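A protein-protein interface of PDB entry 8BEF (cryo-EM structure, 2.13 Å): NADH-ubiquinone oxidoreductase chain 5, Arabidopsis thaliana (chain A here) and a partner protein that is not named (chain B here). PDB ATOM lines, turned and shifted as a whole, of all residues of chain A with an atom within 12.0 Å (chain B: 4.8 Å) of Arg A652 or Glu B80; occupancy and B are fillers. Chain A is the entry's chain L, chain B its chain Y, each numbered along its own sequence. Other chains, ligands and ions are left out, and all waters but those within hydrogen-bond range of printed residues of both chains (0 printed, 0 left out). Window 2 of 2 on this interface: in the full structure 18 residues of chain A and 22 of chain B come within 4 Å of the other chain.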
ATOM      1  N   PHE A 638     -16.735   4.462 -20.476  1.00  0.00           N
ATOM      2  CA  PHE A 638     -15.317   4.134 -20.556  1.00  0.00           C
ATOM      3  C   PHE A 638     -14.451   5.310 -20.123  1.00  0.00           C
ATOM      4  O   PHE A 638     -13.450   5.128 -19.425  1.00  0.00           O
ATOM      5  CB  PHE A 638     -14.954   3.671 -21.970  1.00  0.00           C
ATOM      6  CG  PHE A 638     -13.477   3.706 -22.262  1.00  0.00           C
ATOM      7  CD1 PHE A 638     -12.867   4.859 -22.737  1.00  0.00           C
ATOM      8  CD2 PHE A 638     -12.689   2.595 -22.026  1.00  0.00           C
ATOM      9  CE1 PHE A 638     -11.514   4.893 -22.994  1.00  0.00           C
ATOM     10  CE2 PHE A 638     -11.330   2.625 -22.279  1.00  0.00           C
ATOM     11  CZ  PHE A 638     -10.742   3.775 -22.763  1.00  0.00           C
ATOM     12  N   TRP A 642     -14.320   4.753 -15.327  1.00  0.00           N
ATOM     13  CA  TRP A 642     -13.296   3.728 -15.399  1.00  0.00           C
ATOM     14  C   TRP A 642     -12.235   4.045 -14.345  1.00  0.00           C
ATOM     15  O   TRP A 642     -11.031   3.929 -14.564  1.00  0.00           O
ATOM     16  CB  TRP A 642     -12.733   3.658 -16.816  1.00  0.00           C
ATOM     17  CG  TRP A 642     -12.326   2.300 -17.234  1.00  0.00           C
ATOM     18  CD1 TRP A 642     -11.175   1.654 -16.902  1.00  0.00           C
ATOM     19  CD2 TRP A 642     -13.094   1.378 -18.019  1.00  0.00           C
ATOM     20  NE1 TRP A 642     -11.160   0.400 -17.462  1.00  0.00           N
ATOM     21  CE2 TRP A 642     -12.329   0.206 -18.150  1.00  0.00           C
ATOM     22  CE3 TRP A 642     -14.350   1.436 -18.631  1.00  0.00           C
ATOM     23  CZ2 TRP A 642     -12.777  -0.902 -18.865  1.00  0.00           C
ATOM     24  CZ3 TRP A 642     -14.791   0.337 -19.345  1.00  0.00           C
ATOM     25  CH2 TRP A 642     -14.008  -0.816 -19.456  1.00  0.00           C
ATOM     26  N   LEU A 645     -13.269   0.751 -11.614  1.00  0.00           N
ATOM     27  CA  LEU A 645     -13.477  -0.484 -12.361  1.00  0.00           C
ATOM     28  C   LEU A 645     -12.187  -1.285 -12.479  1.00  0.00           C
ATOM     29  O   LEU A 645     -12.223  -2.519 -12.550  1.00  0.00           O
ATOM     30  CB  LEU A 645     -14.046  -0.172 -13.745  1.00  0.00           C
ATOM     31  CG  LEU A 645     -15.539   0.156 -13.795  1.00  0.00           C
ATOM     32  CD1 LEU A 645     -16.060   0.074 -15.221  1.00  0.00           C
ATOM     33  CD2 LEU A 645     -16.328  -0.766 -12.880  1.00  0.00           C
ATOM     34  N   SER A 646     -11.039  -0.608 -12.474  1.00  0.00           N
ATOM     35  CA  SER A 646      -9.755  -1.262 -12.709  1.00  0.00           C
ATOM     36  C   SER A 646      -9.454  -2.315 -11.649  1.00  0.00           C
ATOM     37  O   SER A 646      -8.608  -3.191 -11.860  1.00  0.00           O
ATOM     38  CB  SER A 646      -8.631  -0.227 -12.753  1.00  0.00           C
ATOM     39  OG  SER A 646      -8.833   0.706 -13.800  1.00  0.00           O
ATOM     40  N   SER A 647     -10.135  -2.235 -10.506  1.00  0.00           N
ATOM     41  CA  SER A 647      -9.951  -3.229  -9.455  1.00  0.00           C
ATOM     42  C   SER A 647     -10.439  -4.607  -9.888  1.00  0.00           C
ATOM     43  O   SER A 647      -9.775  -5.615  -9.621  1.00  0.00           O
ATOM     44  CB  SER A 647     -10.677  -2.785  -8.185  1.00  0.00           C
ATOM     45  OG  SER A 647     -10.186  -1.538  -7.726  1.00  0.00           O
ATOM     46  N   TRP A 648     -11.591  -4.670 -10.555  1.00  0.00           N
ATOM     47  CA  TRP A 648     -12.155  -5.933 -11.009  1.00  0.00           C
ATOM     48  C   TRP A 648     -11.802  -6.272 -12.450  1.00  0.00           C
ATOM     49  O   TRP A 648     -11.785  -7.456 -12.801  1.00  0.00           O
ATOM     50  CB  TRP A 648     -13.681  -5.913 -10.869  1.00  0.00           C
ATOM     51  CG  TRP A 648     -14.182  -6.377  -9.541  1.00  0.00           C
ATOM     52  CD1 TRP A 648     -14.676  -7.612  -9.239  1.00  0.00           C
ATOM     53  CD2 TRP A 648     -14.253  -5.610  -8.336  1.00  0.00           C
ATOM     54  NE1 TRP A 648     -15.047  -7.663  -7.917  1.00  0.00           N
ATOM     55  CE2 TRP A 648     -14.797  -6.446  -7.341  1.00  0.00           C
ATOM     56  CE3 TRP A 648     -13.905  -4.299  -8.000  1.00  0.00           C
ATOM     57  CZ2 TRP A 648     -15.003  -6.013  -6.032  1.00  0.00           C
ATOM     58  CZ3 TRP A 648     -14.112  -3.870  -6.700  1.00  0.00           C
ATOM     59  CH2 TRP A 648     -14.654  -4.724  -5.733  1.00  0.00           C
ATOM     60  N   VAL A 649     -11.523  -5.274 -13.286  1.00  0.00           N
ATOM     61  CA  VAL A 649     -11.267  -5.519 -14.699  1.00  0.00           C
ATOM     62  C   VAL A 649      -9.777  -5.383 -14.970  1.00  0.00           C
ATOM     63  O   VAL A 649      -9.009  -4.949 -14.104  1.00  0.00           O
ATOM     64  CB  VAL A 649     -12.065  -4.559 -15.602  1.00  0.00           C
ATOM     65  CG1 VAL A 649     -13.553  -4.631 -15.290  1.00  0.00           C
ATOM     66  CG2 VAL A 649     -11.531  -3.137 -15.493  1.00  0.00           C
ATOM     67  N   ASP A 650      -9.496  -5.723 -16.262  1.00  0.00           N
ATOM     68  CA  ASP A 650      -8.228  -5.634 -17.008  1.00  0.00           C
ATOM     69  C   ASP A 650      -8.491  -5.262 -18.503  1.00  0.00           C
ATOM     70  O   ASP A 650      -9.485  -5.847 -19.180  1.00  0.00           O
ATOM     71  CB  ASP A 650      -7.676  -7.007 -17.422  1.00  0.00           C
ATOM     72  CG  ASP A 650      -7.402  -7.943 -16.259  1.00  0.00           C
ATOM     73  OD1 ASP A 650      -8.343  -8.216 -15.490  1.00  0.00           O
ATOM     74  OD2 ASP A 650      -6.247  -8.397 -16.136  1.00  0.00           O
ATOM     75  N   ASN A 651      -7.515  -4.609 -19.151  1.00  0.00           N
ATOM     76  CA  ASN A 651      -7.630  -4.166 -20.569  1.00  0.00           C
ATOM     77  C   ASN A 651      -7.587  -5.387 -21.501  1.00  0.00           C
ATOM     78  O   ASN A 651      -8.387  -5.465 -22.502  1.00  0.00           O
ATOM     79  CB  ASN A 651      -6.573  -3.119 -20.926  1.00  0.00           C
ATOM     80  CG  ASN A 651      -6.821  -1.773 -20.278  1.00  0.00           C
ATOM     81  OD1 ASN A 651      -7.951  -1.458 -19.912  1.00  0.00           O
ATOM     82  ND2 ASN A 651      -5.775  -0.973 -20.132  1.00  0.00           N
ATOM     83  N   ARG A 652      -6.815  -6.365 -21.085  1.00  0.00           N
ATOM     84  CA  ARG A 652      -6.730  -7.617 -21.878  1.00  0.00           C
ATOM     85  C   ARG A 652      -8.137  -8.198 -22.057  1.00  0.00           C
ATOM     86  O   ARG A 652      -8.570  -8.380 -23.232  1.00  0.00           O
ATOM     87  CB  ARG A 652      -5.879  -8.580 -21.066  1.00  0.00           C
ATOM     88  CG  ARG A 652      -4.764  -7.906 -20.280  1.00  0.00           C
ATOM     89  CD  ARG A 652      -3.418  -8.114 -20.942  1.00  0.00           C
ATOM     90  NE  ARG A 652      -3.264  -9.493 -21.372  1.00  0.00           N
ATOM     91  CZ  ARG A 652      -2.819 -10.475 -20.596  1.00  0.00           C
ATOM     92  NH1 ARG A 652      -2.473 -10.229 -19.345  1.00  0.00           N
ATOM     93  NH2 ARG A 652      -2.716 -11.699 -21.077  1.00  0.00           N
ATOM     94  N   LEU A 653      -8.826  -8.428 -20.946  1.00  0.00           N
ATOM     95  CA  LEU A 653     -10.156  -9.053 -20.968  1.00  0.00           C
ATOM     96  C   LEU A 653     -11.089  -8.130 -21.793  1.00  0.00           C
ATOM     97  O   LEU A 653     -11.747  -8.667 -22.647  1.00  0.00           O
ATOM     98  CB  LEU A 653     -10.700  -9.264 -19.553  1.00  0.00           C
ATOM     99  CG  LEU A 653      -9.955 -10.282 -18.685  1.00  0.00           C
ATOM    100  CD1 LEU A 653     -10.507 -10.283 -17.268  1.00  0.00           C
ATOM    101  CD2 LEU A 653     -10.033 -11.671 -19.297  1.00  0.00           C
ATOM    102  N   SER A 654     -11.087  -6.831 -21.537  1.00  0.00           N
ATOM    103  CA  SER A 654     -11.874  -5.903 -22.387  1.00  0.00           C
ATOM    104  C   SER A 654     -11.746  -6.249 -23.857  1.00  0.00           C
ATOM    105  O   SER A 654     -12.731  -6.784 -24.398  1.00  0.00           O
ATOM    106  CB  SER A 654     -11.556  -4.425 -22.097  1.00  0.00           C
ATOM    107  OG  SER A 654     -11.711  -3.624 -23.258  1.00  0.00           O
ATOM    108  N   PHE A 655     -10.541  -6.187 -24.424  1.00  0.00           N
ATOM    109  CA  PHE A 655     -10.434  -6.348 -25.888  1.00  0.00           C
ATOM    110  C   PHE A 655     -10.758  -7.799 -26.300  1.00  0.00           C
ATOM    111  O   PHE A 655     -11.425  -7.968 -27.332  1.00  0.00           O
ATOM    112  CB  PHE A 655      -9.105  -5.777 -26.389  1.00  0.00           C
ATOM    113  CG  PHE A 655      -9.007  -4.277 -26.428  1.00  0.00           C
ATOM    114  CD1 PHE A 655      -9.678  -3.547 -27.395  1.00  0.00           C
ATOM    115  CD2 PHE A 655      -8.242  -3.594 -25.498  1.00  0.00           C
ATOM    116  CE1 PHE A 655      -9.587  -2.166 -27.426  1.00  0.00           C
ATOM    117  CE2 PHE A 655      -8.154  -2.213 -25.531  1.00  0.00           C
ATOM    118  CZ  PHE A 655      -8.828  -1.501 -26.492  1.00  0.00           C
ATOM    119  N   ILE A 656     -10.377  -8.784 -25.513  1.00  0.00           N
ATOM    120  CA  ILE A 656     -10.718 -10.205 -25.790  1.00  0.00           C
ATOM    121  C   ILE A 656     -12.226 -10.410 -25.937  1.00  0.00           C
ATOM    122  O   ILE A 656     -12.653 -11.062 -26.902  1.00  0.00           O
ATOM    123  CB  ILE A 656     -10.186 -11.056 -24.641  1.00  0.00           C
ATOM    124  CG1 ILE A 656      -8.678 -10.875 -24.442  1.00  0.00           C
ATOM    125  CG2 ILE A 656     -10.521 -12.533 -24.799  1.00  0.00           C
ATOM    126  CD1 ILE A 656      -7.835 -11.223 -25.641  1.00  0.00           C
ATOM    127  N   LEU A 657     -12.997  -9.884 -24.982  1.00  0.00           N
ATOM    128  CA  LEU A 657     -14.459 -10.136 -25.011  1.00  0.00           C
ATOM    129  C   LEU A 657     -15.012  -9.447 -26.275  1.00  0.00           C
ATOM    130  O   LEU A 657     -15.734 -10.099 -27.020  1.00  0.00           O
ATOM    131  CB  LEU A 657     -14.976  -9.686 -23.635  1.00  0.00           C
ATOM    132  CG  LEU A 657     -14.760 -10.696 -22.517  1.00  0.00           C
ATOM    133  CD1 LEU A 657     -15.267 -10.170 -21.197  1.00  0.00           C
ATOM    134  CD2 LEU A 657     -15.400 -12.037 -22.847  1.00  0.00           C
ATOM    135  N   ILE A 658     -14.471  -8.299 -26.678  1.00  0.00           N
ATOM    136  CA  ILE A 658     -14.955  -7.597 -27.866  1.00  0.00           C
ATOM    137  C   ILE A 658     -14.756  -8.457 -29.107  1.00  0.00           C
ATOM    138  O   ILE A 658     -15.684  -8.661 -29.899  1.00  0.00           O
ATOM    139  CB  ILE A 658     -14.257  -6.233 -28.011  1.00  0.00           C
ATOM    140  CG1 ILE A 658     -14.796  -5.245 -26.974  1.00  0.00           C
ATOM    141  CG2 ILE A 658     -14.447  -5.682 -29.415  1.00  0.00           C
ATOM    142  CD1 ILE A 658     -16.302  -5.229 -26.872  1.00  0.00           C
ATOM    143  N   VAL A 659     -13.544  -8.981 -29.287  1.00  0.00           N
ATOM    144  CA  VAL A 659     -13.268  -9.845 -30.430  1.00  0.00           C
ATOM    145  C   VAL A 659     -14.087 -11.127 -30.339  1.00  0.00           C
ATOM    146  O   VAL A 659     -14.636 -11.604 -31.339  1.00  0.00           O
ATOM    147  CB  VAL A 659     -11.758 -10.134 -30.526  1.00  0.00           C
ATOM    148  CG1 VAL A 659     -11.502 -11.480 -31.184  1.00  0.00           C
ATOM    149  CG2 VAL A 659     -11.056  -9.023 -31.289  1.00  0.00           C
ATOM    150  N   SER A 660     -14.190 -11.697 -29.136  1.00  0.00           N
ATOM    151  CA  SER A 660     -14.938 -12.938 -28.964  1.00  0.00           C
ATOM    152  C   SER A 660     -16.397 -12.786 -29.372  1.00  0.00           C
ATOM    153  O   SER A 660     -17.031 -13.766 -29.775  1.00  0.00           O
ATOM    154  CB  SER A 660     -14.846 -13.413 -27.516  1.00  0.00           C
ATOM    155  OG  SER A 660     -15.810 -14.412 -27.249  1.00  0.00           O
ATOM    156  N   SER A 661     -16.946 -11.571 -29.281  1.00  0.00           N
ATOM    157  CA  SER A 661     -18.341 -11.356 -29.652  1.00  0.00           C
ATOM    158  C   SER A 661     -18.594 -11.687 -31.117  1.00  0.00           C
ATOM    159  O   SER A 661     -19.726 -12.012 -31.491  1.00  0.00           O
ATOM    160  CB  SER A 661     -18.748  -9.912 -29.366  1.00  0.00           C
ATOM    161  OG  SER A 661     -18.432  -9.544 -28.036  1.00  0.00           O
ATOM    162  N   VAL B  75     -11.607 -18.476 -17.959  1.00  0.00           N
ATOM    163  CA  VAL B  75     -10.645 -19.443 -18.480  1.00  0.00           C
ATOM    164  C   VAL B  75      -9.408 -18.734 -19.022  1.00  0.00           C
ATOM    165  O   VAL B  75      -8.282 -19.220 -18.864  1.00  0.00           O
ATOM    166  CB  VAL B  75     -11.313 -20.332 -19.547  1.00  0.00           C
ATOM    167  CG1 VAL B  75     -10.296 -20.833 -20.558  1.00  0.00           C
ATOM    168  CG2 VAL B  75     -12.037 -21.493 -18.890  1.00  0.00           C
ATOM    169  N   TYR B  76      -9.590 -17.569 -19.653  1.00  0.00           N
ATOM    170  CA  TYR B  76      -8.457 -16.819 -20.187  1.00  0.00           C
ATOM    171  C   TYR B  76      -7.420 -16.534 -19.107  1.00  0.00           C
ATOM    172  O   TYR B  76      -6.271 -16.987 -19.192  1.00  0.00           O
ATOM    173  CB  TYR B  76      -8.962 -15.518 -20.815  1.00  0.00           C
ATOM    174  CG  TYR B  76      -7.879 -14.614 -21.344  1.00  0.00           C
ATOM    175  CD1 TYR B  76      -6.906 -15.095 -22.205  1.00  0.00           C
ATOM    176  CD2 TYR B  76      -7.834 -13.276 -20.987  1.00  0.00           C
ATOM    177  CE1 TYR B  76      -5.917 -14.266 -22.694  1.00  0.00           C
ATOM    178  CE2 TYR B  76      -6.853 -12.441 -21.472  1.00  0.00           C
ATOM    179  CZ  TYR B  76      -5.895 -12.940 -22.324  1.00  0.00           C
ATOM    180  OH  TYR B  76      -4.911 -12.109 -22.808  1.00  0.00           O
ATOM    181  N   ILE B  77      -7.817 -15.794 -18.070  1.00  0.00           N
ATOM    182  CA  ILE B  77      -6.884 -15.443 -17.007  1.00  0.00           C
ATOM    183  C   ILE B  77      -6.434 -16.678 -16.241  1.00  0.00           C
ATOM    184  O   ILE B  77      -5.282 -16.751 -15.807  1.00  0.00           O
ATOM    185  CB  ILE B  77      -7.503 -14.393 -16.067  1.00  0.00           C
ATOM    186  CG1 ILE B  77      -7.712 -13.075 -16.816  1.00  0.00           C
ATOM    187  CG2 ILE B  77      -6.630 -14.207 -14.828  1.00  0.00           C
ATOM    188  CD1 ILE B  77      -8.552 -12.058 -16.070  1.00  0.00           C
ATOM    189  N   GLY B  78      -7.313 -17.667 -16.063  1.00  0.00           N
ATOM    190  CA  GLY B  78      -6.920 -18.858 -15.333  1.00  0.00           C
ATOM    191  C   GLY B  78      -5.794 -19.611 -16.012  1.00  0.00           C
ATOM    192  O   GLY B  78      -4.797 -19.961 -15.380  1.00  0.00           O
ATOM    193  N   VAL B  79      -5.929 -19.853 -17.316  1.00  0.00           N
ATOM    194  CA  VAL B  79      -4.874 -20.545 -18.044  1.00  0.00           C
ATOM    195  C   VAL B  79      -3.637 -19.663 -18.147  1.00  0.00           C
ATOM    196  O   VAL B  79      -2.505 -20.154 -18.072  1.00  0.00           O
ATOM    197  CB  VAL B  79      -5.374 -20.996 -19.427  1.00  0.00           C
ATOM    198  CG1 VAL B  79      -4.211 -21.497 -20.270  1.00  0.00           C
ATOM    199  CG2 VAL B  79      -6.429 -22.076 -19.276  1.00  0.00           C
ATOM    200  N   GLU B  80      -3.827 -18.348 -18.295  1.00  0.00           N
ATOM    201  CA  GLU B  80      -2.685 -17.442 -18.341  1.00  0.00           C
ATOM    202  C   GLU B  80      -1.852 -17.536 -17.069  1.00  0.00           C
ATOM    203  O   GLU B  80      -0.620 -17.633 -17.123  1.00  0.00           O
ATOM    204  CB  GLU B  80      -3.168 -16.009 -18.557  1.00  0.00           C
ATOM    205  CG  GLU B  80      -2.082 -14.960 -18.380  1.00  0.00           C
ATOM    206  CD  GLU B  80      -2.642 -13.559 -18.269  1.00  0.00           C
ATOM    207  OE1 GLU B  80      -3.840 -13.371 -18.568  1.00  0.00           O
ATOM    208  OE2 GLU B  80      -1.886 -12.643 -17.883  1.00  0.00           O
ATOM    209  N   GLN B  81      -2.510 -17.511 -15.909  1.00  0.00           N
ATOM    210  CA  GLN B  81      -1.782 -17.584 -14.648  1.00  0.00           C
ATOM    211  C   GLN B  81      -1.230 -18.983 -14.409  1.00  0.00           C
ATOM    212  O   GLN B  81      -0.117 -19.138 -13.897  1.00  0.00           O
ATOM    213  CB  GLN B  81      -2.683 -17.150 -13.492  1.00  0.00           C
ATOM    214  CG  GLN B  81      -3.305 -15.762 -13.644  1.00  0.00           C
ATOM    215  CD  GLN B  81      -2.289 -14.635 -13.726  1.00  0.00           C
ATOM    216  OE1 GLN B  81      -1.516 -14.538 -14.680  1.00  0.00           O
ATOM    217  NE2 GLN B  81      -2.293 -13.766 -12.722  1.00  0.00           N
ATOM    218  N   LEU B  82      -1.988 -20.017 -14.785  1.00  0.00           N
ATOM    219  CA  LEU B  82      -1.511 -21.387 -14.669  1.00  0.00           C
ATOM    220  C   LEU B  82      -0.365 -21.688 -15.624  1.00  0.00           C
ATOM    221  O   LEU B  82       0.283 -22.730 -15.480  1.00  0.00           O
ATOM    222  CB  LEU B  82      -2.663 -22.360 -14.915  1.00  0.00           C
ATOM    223  CG  LEU B  82      -2.717 -23.602 -14.024  1.00  0.00           C
ATOM    224  CD1 LEU B  82      -2.227 -23.279 -12.621  1.00  0.00           C
ATOM    225  CD2 LEU B  82      -4.125 -24.176 -13.986  1.00  0.00           C
ATOM    226  N   VAL B  83      -0.109 -20.816 -16.595  1.00  0.00           N
ATOM    227  CA  VAL B  83       1.045 -20.971 -17.473  1.00  0.00           C
ATOM    228  C   VAL B  83       2.253 -20.217 -16.930  1.00  0.00           C
ATOM    229  O   VAL B  83       3.373 -20.734 -16.953  1.00  0.00           O
ATOM    230  CB  VAL B  83       0.685 -20.518 -18.902  1.00  0.00           C
ATOM    231  CG1 VAL B  83       1.939 -20.205 -19.699  1.00  0.00           C
ATOM    232  CG2 VAL B  83      -0.131 -21.593 -19.606  1.00  0.00           C
ATOM    233  N   GLN B  84       2.053 -19.006 -16.414  1.00  0.00           N
ATOM    234  CA  GLN B  84       3.162 -18.225 -15.877  1.00  0.00           C
ATOM    235  C   GLN B  84       3.519 -18.605 -14.445  1.00  0.00           C
ATOM    236  O   GLN B  84       4.468 -18.041 -13.893  1.00  0.00           O
ATOM    237  CB  GLN B  84       2.846 -16.729 -15.952  1.00  0.00           C
ATOM    238  CG  GLN B  84       2.009 -16.191 -14.807  1.00  0.00           C
ATOM    239  CD  GLN B  84       2.091 -14.682 -14.701  1.00  0.00           C
ATOM    240  OE1 GLN B  84       1.185 -13.968 -15.128  1.00  0.00           O
ATOM    241  NE2 GLN B  84       3.185 -14.188 -14.135  1.00  0.00           N
ATOM    242  N   ASN B  94       2.702 -16.402 -22.390  1.00  0.00           N
ATOM    243  CA  ASN B  94       1.675 -16.666 -21.395  1.00  0.00           C
ATOM    244  C   ASN B  94       0.564 -15.637 -21.548  1.00  0.00           C
ATOM    245  O   ASN B  94       0.806 -14.427 -21.491  1.00  0.00           O
ATOM    246  CB  ASN B  94       2.266 -16.635 -19.985  1.00  0.00           C
ATOM    247  CG  ASN B  94       2.995 -15.345 -19.684  1.00  0.00           C
ATOM    248  OD1 ASN B  94       4.192 -15.220 -19.941  1.00  0.00           O
ATOM    249  ND2 ASN B  94       2.276 -14.372 -19.135  1.00  0.00           N
ATOM    250  N   GLY B  95      -0.656 -16.120 -21.755  1.00  0.00           N
ATOM    251  CA  GLY B  95      -1.766 -15.292 -22.159  1.00  0.00           C
ATOM    252  C   GLY B  95      -2.194 -15.499 -23.596  1.00  0.00           C
ATOM    253  O   GLY B  95      -3.394 -15.450 -23.884  1.00  0.00           O
ATOM    254  N   GLY B  98      -3.506 -18.901 -23.120  1.00  0.00           N
ATOM    255  CA  GLY B  98      -4.796 -18.756 -22.463  1.00  0.00           C
ATOM    256  C   GLY B  98      -5.873 -18.248 -23.399  1.00  0.00           C
ATOM    257  O   GLY B  98      -7.001 -18.750 -23.401  1.00  0.00           O
ATOM    258  N   ILE B 131      -1.165  -7.561 -27.082  1.00  0.00           N
ATOM    259  CA  ILE B 131      -1.102  -6.875 -25.767  1.00  0.00           C
ATOM    260  C   ILE B 131       0.051  -7.444 -24.916  1.00  0.00           C
ATOM    261  O   ILE B 131       0.907  -6.621 -24.523  1.00  0.00           O
ATOM    262  CB  ILE B 131      -2.468  -6.915 -25.060  1.00  0.00           C
ATOM    263  CG1 ILE B 131      -3.551  -6.308 -25.955  1.00  0.00           C
ATOM    264  CG2 ILE B 131      -2.396  -6.206 -23.722  1.00  0.00           C
ATOM    265  CD1 ILE B 131      -4.888  -6.138 -25.287  1.00  0.00           C
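Of the printed residues of chain B, Asp A650 touches Ile B77.
Asn A651 touches none of the printed residues of chain B.
Of chain B, only Tyr B76 (2.8 Å), Glu B80 (2.9 Å), Gly B95 (3.9 Å) and Ile B131 (3.5 Å) come within 4 Å of Arg A652.
Printed residues of chain B within 4 Å of Leu A653: Tyr B76 (3.2 Å) and Ile B77 (2.9 Å).
Of the printed residues of chain B, Ile A656 touches Tyr B76 (3.8 Å).
No residue of chain A comes within 4 Å of Gly B78.
No residue of chain A comes within 4 Å of Val B79.
Glu B80 touches one residue of chain A.
No residue of chain A comes within 4 Å of Gln B81.
No residue of chain A comes within 4 Å of Val B83.
No residue of chain A comes within 4 Å of Gln B84.
No residue of chain A comes within 4 Å of Asn B94.
Gly B95 touches just one residue of chain A: Arg A652.
No residue of chain A comes within 4 Å of Gly B98.
Of chain A, only Arg A652 comes within 4 Å of Ile B131.
The nearest residue of chain B that does not touch Arg A652 is Asn B94 (4.5 Å).
The nearest residue of chain A that does not touch Glu B80 is Asp A650 (6.0 Å).
Among the printed residues, merely in contact across the chains: Leu A653 with Ile B77 (2.9 Å), Leu A653 with Tyr B76 (3.2 Å), Arg A652 with Ile B131 (3.5 Å), Ile A656 with Tyr B76 (3.8 Å), Arg A652 with Gly B95 (3.9 Å) and Asp A650 with Ile B77 (3.9 Å).
Of the 19 printed residues of chain A, 4 touch a printed residue of chain B.
Of the 14 printed residues of chain B, 5 touch a printed residue of chain A.
Hydrophobic or aromatic side chains of chain B that line the printed part of chain A: Tyr B76, Ile B77 and Ile B131.
Among the printed residues, 8 pairs touch across the chains.
Among the printed residues, Asp or Glu carboxylates within 4 Å of a Lys or Arg side-chain nitrogen of the other chain: Arg A652 with Glu B80 (2.9 Å).
The guanidinium group (NH2) of Arg A652 is in hydrogen-bond range of the side-chain hydroxyl (OH) of Tyr B76, at 2.8 Å.
OE2 of Glu B80 lies within salt-bridge range of NH1 of Arg A652, at 2.9 Å.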
